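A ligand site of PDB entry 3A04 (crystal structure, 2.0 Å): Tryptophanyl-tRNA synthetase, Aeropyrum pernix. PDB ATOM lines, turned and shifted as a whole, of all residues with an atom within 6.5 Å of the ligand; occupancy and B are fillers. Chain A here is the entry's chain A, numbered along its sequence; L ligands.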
ATOM      1  N   LEU A 283      19.551   3.735   8.914  1.00  0.00           N
ATOM      2  CA  LEU A 283      18.373   4.214   9.653  1.00  0.00           C
ATOM      3  C   LEU A 283      17.935   3.278  10.794  1.00  0.00           C
ATOM      4  O   LEU A 283      17.870   2.024  10.643  1.00  0.00           O
ATOM      5  CB  LEU A 283      17.207   4.494   8.686  1.00  0.00           C
ATOM      6  CG  LEU A 283      17.578   5.437   7.525  1.00  0.00           C
ATOM      7  CD1 LEU A 283      16.377   5.875   6.658  1.00  0.00           C
ATOM      8  CD2 LEU A 283      18.360   6.659   8.001  1.00  0.00           C
ATOM      9  N   THR A 284      17.637   3.878  11.934  1.00  0.00           N
ATOM     10  CA  THR A 284      17.208   3.135  13.104  1.00  0.00           C
ATOM     11  C   THR A 284      15.827   3.599  13.551  1.00  0.00           C
ATOM     12  O   THR A 284      15.285   4.571  13.023  1.00  0.00           O
ATOM     13  CB  THR A 284      18.165   3.410  14.301  1.00  0.00           C
ATOM     14  OG1 THR A 284      18.039   4.790  14.686  1.00  0.00           O
ATOM     15  CG2 THR A 284      19.575   3.130  13.888  1.00  0.00           C
ATOM     16  N   GLY A 285      15.246   2.888  14.507  1.00  0.00           N
ATOM     17  CA  GLY A 285      14.109   3.414  15.259  1.00  0.00           C
ATOM     18  C   GLY A 285      14.522   4.214  16.501  1.00  0.00           C
ATOM     19  O   GLY A 285      13.851   4.149  17.497  1.00  0.00           O
ATOM     20  N   GLY A 286      15.665   4.905  16.454  1.00  0.00           N
ATOM     21  CA  GLY A 286      16.189   5.689  17.592  1.00  0.00           C
ATOM     22  C   GLY A 286      15.448   7.034  17.713  1.00  0.00           C
ATOM     23  O   GLY A 286      14.533   7.324  16.907  1.00  0.00           O
ATOM     24  N   ARG A 287      15.779   7.833  18.727  1.00  0.00           N
ATOM     25  CA  ARG A 287      14.990   9.052  18.989  1.00  0.00           C
ATOM     26  C   ARG A 287      15.893  10.247  18.939  1.00  0.00           C
ATOM     27  O   ARG A 287      17.106  10.109  18.671  1.00  0.00           O
ATOM     28  CB  ARG A 287      14.220   9.011  20.332  1.00  0.00           C
ATOM     29  CG  ARG A 287      13.441   7.724  20.677  1.00  0.00           C
ATOM     30  CD  ARG A 287      11.894   7.684  20.356  1.00  0.00           C
ATOM     31  NE  ARG A 287      11.369   6.455  20.997  1.00  0.00           N
ATOM     32  CZ  ARG A 287      10.125   5.948  20.910  1.00  0.00           C
ATOM     33  NH1 ARG A 287       9.170   6.536  20.193  1.00  0.00           N
ATOM     34  NH2 ARG A 287       9.846   4.797  21.548  1.00  0.00           N
ATOM     35  N   GLN A 293      15.723   8.708  24.286  1.00  0.00           N
ATOM     36  CA  GLN A 293      15.803   7.257  24.075  1.00  0.00           C
ATOM     37  C   GLN A 293      15.714   6.522  25.413  1.00  0.00           C
ATOM     38  O   GLN A 293      14.979   5.537  25.527  1.00  0.00           O
ATOM     39  CB  GLN A 293      17.079   6.887  23.307  1.00  0.00           C
ATOM     40  CG  GLN A 293      17.388   5.348  23.198  1.00  0.00           C
ATOM     41  CD  GLN A 293      16.718   4.621  22.022  1.00  0.00           C
ATOM     42  OE1 GLN A 293      16.031   5.234  21.199  1.00  0.00           O
ATOM     43  NE2 GLN A 293      16.899   3.303  21.967  1.00  0.00           N
ATOM     44  N   GLY A 297      12.663   4.346  25.196  1.00  0.00           N
ATOM     45  CA  GLY A 297      13.283   3.275  24.403  1.00  0.00           C
ATOM     46  C   GLY A 297      13.165   3.500  22.895  1.00  0.00           C
ATOM     47  O   GLY A 297      12.832   4.600  22.433  1.00  0.00           O
ATOM     48  N   GLY A 298      13.464   2.458  22.120  1.00  0.00           N
ATOM     49  CA  GLY A 298      13.441   2.597  20.685  1.00  0.00           C
ATOM     50  C   GLY A 298      12.341   1.830  19.988  1.00  0.00           C
ATOM     51  O   GLY A 298      11.466   1.171  20.633  1.00  0.00           O
ATOM     52  N   VAL A 299      12.361   1.891  18.663  1.00  0.00           N
ATOM     53  CA  VAL A 299      11.359   1.243  17.869  1.00  0.00           C
ATOM     54  C   VAL A 299      12.026   0.229  16.898  1.00  0.00           C
ATOM     55  O   VAL A 299      12.352   0.571  15.754  1.00  0.00           O
ATOM     56  CB  VAL A 299      10.443   2.323  17.165  1.00  0.00           C
ATOM     57  CG1 VAL A 299       9.259   1.663  16.360  1.00  0.00           C
ATOM     58  CG2 VAL A 299       9.918   3.381  18.221  1.00  0.00           C
ATOM     59  N   PRO A 300      12.267  -1.014  17.380  1.00  0.00           N
ATOM     60  CA  PRO A 300      12.936  -2.046  16.543  1.00  0.00           C
ATOM     61  C   PRO A 300      12.153  -2.426  15.263  1.00  0.00           C
ATOM     62  O   PRO A 300      12.767  -2.713  14.239  1.00  0.00           O
ATOM     63  CB  PRO A 300      13.054  -3.266  17.499  1.00  0.00           C
ATOM     64  CG  PRO A 300      13.122  -2.646  18.918  1.00  0.00           C
ATOM     65  CD  PRO A 300      12.137  -1.453  18.794  1.00  0.00           C
ATOM     66  N   CYS A 303      13.547  -0.469  12.443  1.00  0.00           N
ATOM     67  CA  CYS A 303      14.983  -0.204  12.558  1.00  0.00           C
ATOM     68  C   CYS A 303      15.700  -1.186  11.645  1.00  0.00           C
ATOM     69  O   CYS A 303      15.519  -2.422  11.773  1.00  0.00           O
ATOM     70  CB  CYS A 303      15.444  -0.470  13.995  1.00  0.00           C
ATOM     71  SG  CYS A 303      17.182  -0.290  14.120  1.00  0.00           S
ATOM     72  N   SER A 304      16.498  -0.669  10.748  1.00  0.00           N
ATOM     73  CA  SER A 304      17.207  -1.554   9.797  1.00  0.00           C
ATOM     74  C   SER A 304      18.427  -2.260  10.470  1.00  0.00           C
ATOM     75  O   SER A 304      18.937  -3.254   9.980  1.00  0.00           O
ATOM     76  CB  SER A 304      17.616  -0.725   8.578  1.00  0.00           C
ATOM     77  OG  SER A 304      18.727   0.060   8.913  1.00  0.00           O
ATOM     78  N   VAL A 305      18.870  -1.766  11.639  1.00  0.00           N
ATOM     79  CA  VAL A 305      19.944  -2.462  12.385  1.00  0.00           C
ATOM     80  C   VAL A 305      19.374  -3.728  13.026  1.00  0.00           C
ATOM     81  O   VAL A 305      19.931  -4.836  12.892  1.00  0.00           O
ATOM     82  CB  VAL A 305      20.541  -1.551  13.488  1.00  0.00           C
ATOM     83  CG1 VAL A 305      21.566  -2.387  14.370  1.00  0.00           C
ATOM     84  CG2 VAL A 305      21.194  -0.306  12.844  1.00  0.00           C
ATOM     85  N   TYR A 306      18.222  -3.548  13.656  1.00  0.00           N
ATOM     86  CA  TYR A 306      17.529  -4.645  14.264  1.00  0.00           C
ATOM     87  C   TYR A 306      17.148  -5.698  13.203  1.00  0.00           C
ATOM     88  O   TYR A 306      17.267  -6.898  13.442  1.00  0.00           O
ATOM     89  CB  TYR A 306      16.260  -4.164  15.018  1.00  0.00           C
ATOM     90  CG  TYR A 306      15.515  -5.318  15.638  1.00  0.00           C
ATOM     91  CD1 TYR A 306      16.063  -6.037  16.730  1.00  0.00           C
ATOM     92  CD2 TYR A 306      14.304  -5.792  15.088  1.00  0.00           C
ATOM     93  CE1 TYR A 306      15.387  -7.201  17.275  1.00  0.00           C
ATOM     94  CE2 TYR A 306      13.626  -6.946  15.624  1.00  0.00           C
ATOM     95  CZ  TYR A 306      14.178  -7.621  16.721  1.00  0.00           C
ATOM     96  OH  TYR A 306      13.508  -8.715  17.260  1.00  0.00           O
ATOM     97  N   ASP A 309      20.167  -7.750  12.467  1.00  0.00           N
ATOM     98  CA  ASP A 309      20.302  -8.795  13.519  1.00  0.00           C
ATOM     99  C   ASP A 309      19.316  -9.940  13.347  1.00  0.00           C
ATOM    100  O   ASP A 309      19.654 -11.091  13.453  1.00  0.00           O
ATOM    101  CB  ASP A 309      20.030  -8.148  14.923  1.00  0.00           C
ATOM    102  CG  ASP A 309      21.179  -7.233  15.359  1.00  0.00           C
ATOM    103  OD1 ASP A 309      22.293  -7.414  14.874  1.00  0.00           O
ATOM    104  OD2 ASP A 309      20.931  -6.331  16.165  1.00  0.00           O
ATOM    105  N   ILE A 323      18.241  -7.976  22.332  1.00  0.00           N
ATOM    106  CA  ILE A 323      18.331  -6.669  21.718  1.00  0.00           C
ATOM    107  C   ILE A 323      16.969  -5.974  21.698  1.00  0.00           C
ATOM    108  O   ILE A 323      16.875  -4.783  21.959  1.00  0.00           O
ATOM    109  CB  ILE A 323      18.890  -6.669  20.235  1.00  0.00           C
ATOM    110  CG1 ILE A 323      20.360  -7.079  20.178  1.00  0.00           C
ATOM    111  CG2 ILE A 323      18.685  -5.244  19.626  1.00  0.00           C
ATOM    112  CD1 ILE A 323      21.307  -6.235  21.075  1.00  0.00           C
ATOM    113  N   TYR A 324      15.926  -6.719  21.293  1.00  0.00           N
ATOM    114  CA  TYR A 324      14.593  -6.149  21.159  1.00  0.00           C
ATOM    115  C   TYR A 324      14.098  -5.588  22.528  1.00  0.00           C
ATOM    116  O   TYR A 324      13.630  -4.447  22.613  1.00  0.00           O
ATOM    117  CB  TYR A 324      13.631  -7.224  20.650  1.00  0.00           C
ATOM    118  CG  TYR A 324      12.222  -6.760  20.475  1.00  0.00           C
ATOM    119  CD1 TYR A 324      11.852  -6.090  19.312  1.00  0.00           C
ATOM    120  CD2 TYR A 324      11.243  -6.981  21.464  1.00  0.00           C
ATOM    121  CE1 TYR A 324      10.565  -5.644  19.085  1.00  0.00           C
ATOM    122  CE2 TYR A 324       9.913  -6.529  21.264  1.00  0.00           C
ATOM    123  CZ  TYR A 324       9.579  -5.857  20.073  1.00  0.00           C
ATOM    124  OH  TYR A 324       8.328  -5.381  19.827  1.00  0.00           O
ATOM    125  N   SER A 326      15.838  -4.954  25.395  1.00  0.00           N
ATOM    126  CA  SER A 326      16.666  -3.827  25.823  1.00  0.00           C
ATOM    127  C   SER A 326      16.339  -2.508  25.152  1.00  0.00           C
ATOM    128  O   SER A 326      16.155  -1.479  25.837  1.00  0.00           O
ATOM    129  CB  SER A 326      18.160  -4.152  25.739  1.00  0.00           C
ATOM    130  OG  SER A 326      18.396  -5.419  26.350  1.00  0.00           O
ATOM    131  N   CYS A 327      16.254  -2.510  23.811  1.00  0.00           N
ATOM    132  CA  CYS A 327      15.815  -1.328  23.082  1.00  0.00           C
ATOM    133  C   CYS A 327      14.394  -0.901  23.485  1.00  0.00           C
ATOM    134  O   CYS A 327      14.113   0.295  23.587  1.00  0.00           O
ATOM    135  CB  CYS A 327      15.854  -1.587  21.579  1.00  0.00           C
ATOM    136  SG  CYS A 327      15.155  -0.241  20.644  1.00  0.00           S
ATOM    137  N   ARG A 328      13.491  -1.855  23.657  1.00  0.00           N
ATOM    138  CA  ARG A 328      12.106  -1.516  24.033  1.00  0.00           C
ATOM    139  C   ARG A 328      11.940  -1.169  25.519  1.00  0.00           C
ATOM    140  O   ARG A 328      10.885  -0.681  25.923  1.00  0.00           O
ATOM    141  CB  ARG A 328      11.143  -2.637  23.671  1.00  0.00           C
ATOM    142  CG  ARG A 328      10.850  -2.716  22.189  1.00  0.00           C
ATOM    143  CD  ARG A 328       9.462  -3.222  21.951  1.00  0.00           C
ATOM    144  NE  ARG A 328       8.449  -2.299  22.464  1.00  0.00           N
ATOM    145  CZ  ARG A 328       7.184  -2.638  22.720  1.00  0.00           C
ATOM    146  NH1 ARG A 328       6.754  -3.877  22.503  1.00  0.00           N
ATOM    147  NH2 ARG A 328       6.352  -1.708  23.195  1.00  0.00           N
ATOM    148  N   ILE A 332      19.347   0.587  25.942  1.00  0.00           N
ATOM    149  CA  ILE A 332      20.389   0.587  24.962  1.00  0.00           C
ATOM    150  C   ILE A 332      20.214   1.745  23.990  1.00  0.00           C
ATOM    151  O   ILE A 332      19.099   2.040  23.580  1.00  0.00           O
ATOM    152  CB  ILE A 332      20.482  -0.825  24.210  1.00  0.00           C
ATOM    153  CG1 ILE A 332      21.779  -0.943  23.392  1.00  0.00           C
ATOM    154  CG2 ILE A 332      19.238  -1.106  23.316  1.00  0.00           C
ATOM    155  CD1 ILE A 332      21.891  -2.285  22.674  1.00  0.00           C
ATOM    156  N   LEU A 333      21.325   2.381  23.638  1.00  0.00           N
ATOM    157  CA  LEU A 333      21.350   3.446  22.636  1.00  0.00           C
ATOM    158  C   LEU A 333      21.820   2.878  21.287  1.00  0.00           C
ATOM    159  O   LEU A 333      22.540   1.872  21.245  1.00  0.00           O
ATOM    160  CB  LEU A 333      22.272   4.576  23.098  1.00  0.00           C
ATOM    161  CG  LEU A 333      21.937   5.298  24.440  1.00  0.00           C
ATOM    162  CD1 LEU A 333      22.836   6.539  24.616  1.00  0.00           C
ATOM    163  CD2 LEU A 333      20.471   5.634  24.554  1.00  0.00           C
ATOM    164  N   CYS A 334      21.485   3.580  20.199  1.00  0.00           N
ATOM    165  CA  CYS A 334      21.775   3.121  18.838  1.00  0.00           C
ATOM    166  C   CYS A 334      23.261   3.002  18.521  1.00  0.00           C
ATOM    167  O   CYS A 334      23.679   2.128  17.761  1.00  0.00           O
ATOM    168  CB  CYS A 334      21.091   4.057  17.830  1.00  0.00           C
ATOM    169  SG  CYS A 334      19.266   3.916  17.887  1.00  0.00           S
ATOM    170  N   GLY A 335      24.075   3.875  19.106  1.00  0.00           N
ATOM    171  CA  GLY A 335      25.510   3.798  18.921  1.00  0.00           C
ATOM    172  C   GLY A 335      26.027   2.449  19.428  1.00  0.00           C
ATOM    173  O   GLY A 335      26.846   1.801  18.757  1.00  0.00           O
ATOM    174  N   CYS A 337      24.214  -0.329  20.094  1.00  0.00           N
ATOM    175  CA  CYS A 337      23.527  -1.326  19.314  1.00  0.00           C
ATOM    176  C   CYS A 337      24.171  -1.578  17.943  1.00  0.00           C
ATOM    177  O   CYS A 337      24.321  -2.741  17.544  1.00  0.00           O
ATOM    178  CB  CYS A 337      22.115  -0.892  19.138  1.00  0.00           C
ATOM    179  SG  CYS A 337      21.014  -2.251  18.704  1.00  0.00           S
ATOM    180  N   LYS A 338      24.562  -0.491  17.255  1.00  0.00           N
ATOM    181  CA  LYS A 338      25.298  -0.567  16.004  1.00  0.00           C
ATOM    182  C   LYS A 338      26.648  -1.185  16.188  1.00  0.00           C
ATOM    183  O   LYS A 338      27.042  -1.965  15.357  1.00  0.00           O
ATOM    184  CB  LYS A 338      25.496   0.817  15.366  1.00  0.00           C
ATOM    185  CG  LYS A 338      24.140   1.320  14.775  1.00  0.00           C
ATOM    186  CD  LYS A 338      24.238   2.770  14.265  1.00  0.00           C
ATOM    187  CE  LYS A 338      23.039   3.073  13.255  1.00  0.00           C
ATOM    188  NZ  LYS A 338      23.034   4.504  12.817  1.00  0.00           N
HETATM  189 FE1  LIG L   1      19.240  -0.875  18.275  1.00  0.00          FE
HETATM  190 FE2  LIG L   1      16.769  -0.019  19.121  1.00  0.00          FE
HETATM  191 FE3  LIG L   1      18.588   1.763  18.069  1.00  0.00          FE
HETATM  192 FE4  LIG L   1      17.526  -0.169  16.438  1.00  0.00          FE
HETATM  193  S1  LIG L   1      16.356   1.580  17.575  1.00  0.00           S
HETATM  194  S2  LIG L   1      19.703   0.447  16.527  1.00  0.00           S
HETATM  195  S3  LIG L   1      17.253  -1.910  17.810  1.00  0.00           S
HETATM  196  S4  LIG L   1      18.766   0.589  20.078  1.00  0.00           S
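CG2 of Thr 284 touches S2 of the ligand, at 3.8 Å.
Val 305 touches the ligand.
Tyr 306 touches the ligand (CB to S3, 3.7 Å).
Ile 332 touches the ligand (CG2 to S4, 3.7 Å).
Hydrophobic or aromatic side chains that line the ligand: Val 305, Tyr 306 and Ile 332.
Of the 26 residues printed, 11 come within 4 Å of the ligand.
O of Cys 327 sits at hydrogen-bond distance from N of Gly 298 (2.7 Å).
The side-chain hydroxyl of Thr 284 sits close to the side-chain sulfur of Cys 334, at 3.5 Å.
The side-chain sulfur (SG) of Cys 303 sits close to the backbone NH (N) of Gly 285 (3.7 Å).
The side-chain sulfur (SG) of Cys 303 lies close to the backbone NH (N) of Tyr 306 (3.5 Å).
SG of Cys 303 sits close to N of Val 305 (3.3 Å).
O of Gly 285 sits at hydrogen-bond distance from N of Val 299 (2.9 Å).
The backbone NH (N) of Gly 286 is in hydrogen-bond range of the side-chain hydroxyl (OG1) of Thr 284.
O of Gly 297 lies close to OE1 of Gln 293 (3.5 Å).
The side-chain sulfur of Cys 327 is bound to an iron atom (FE2) of the ligand (2.2 Å).
An iron atom (FE3) of the ligand is bound by the side-chain sulfur of Cys 334, 2.3 Å away.
SG of Cys 337 binds FE1 of the ligand, at 2.3 Å.
The side-chain sulfur (SG) of Cys 303 is bound to an iron atom (FE4) of the ligand, 2.3 Å away.
The backbone NH (N) of Gly 285 sits close to a sulfur (S1) of the ligand, at 3.5 Å.
The backbone NH (N) of Gly 286 lies close to a sulfur (S1) of the ligand (3.6 Å).
NE2 of Gln 293 lies close to S4 of the ligand (3.8 Å).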
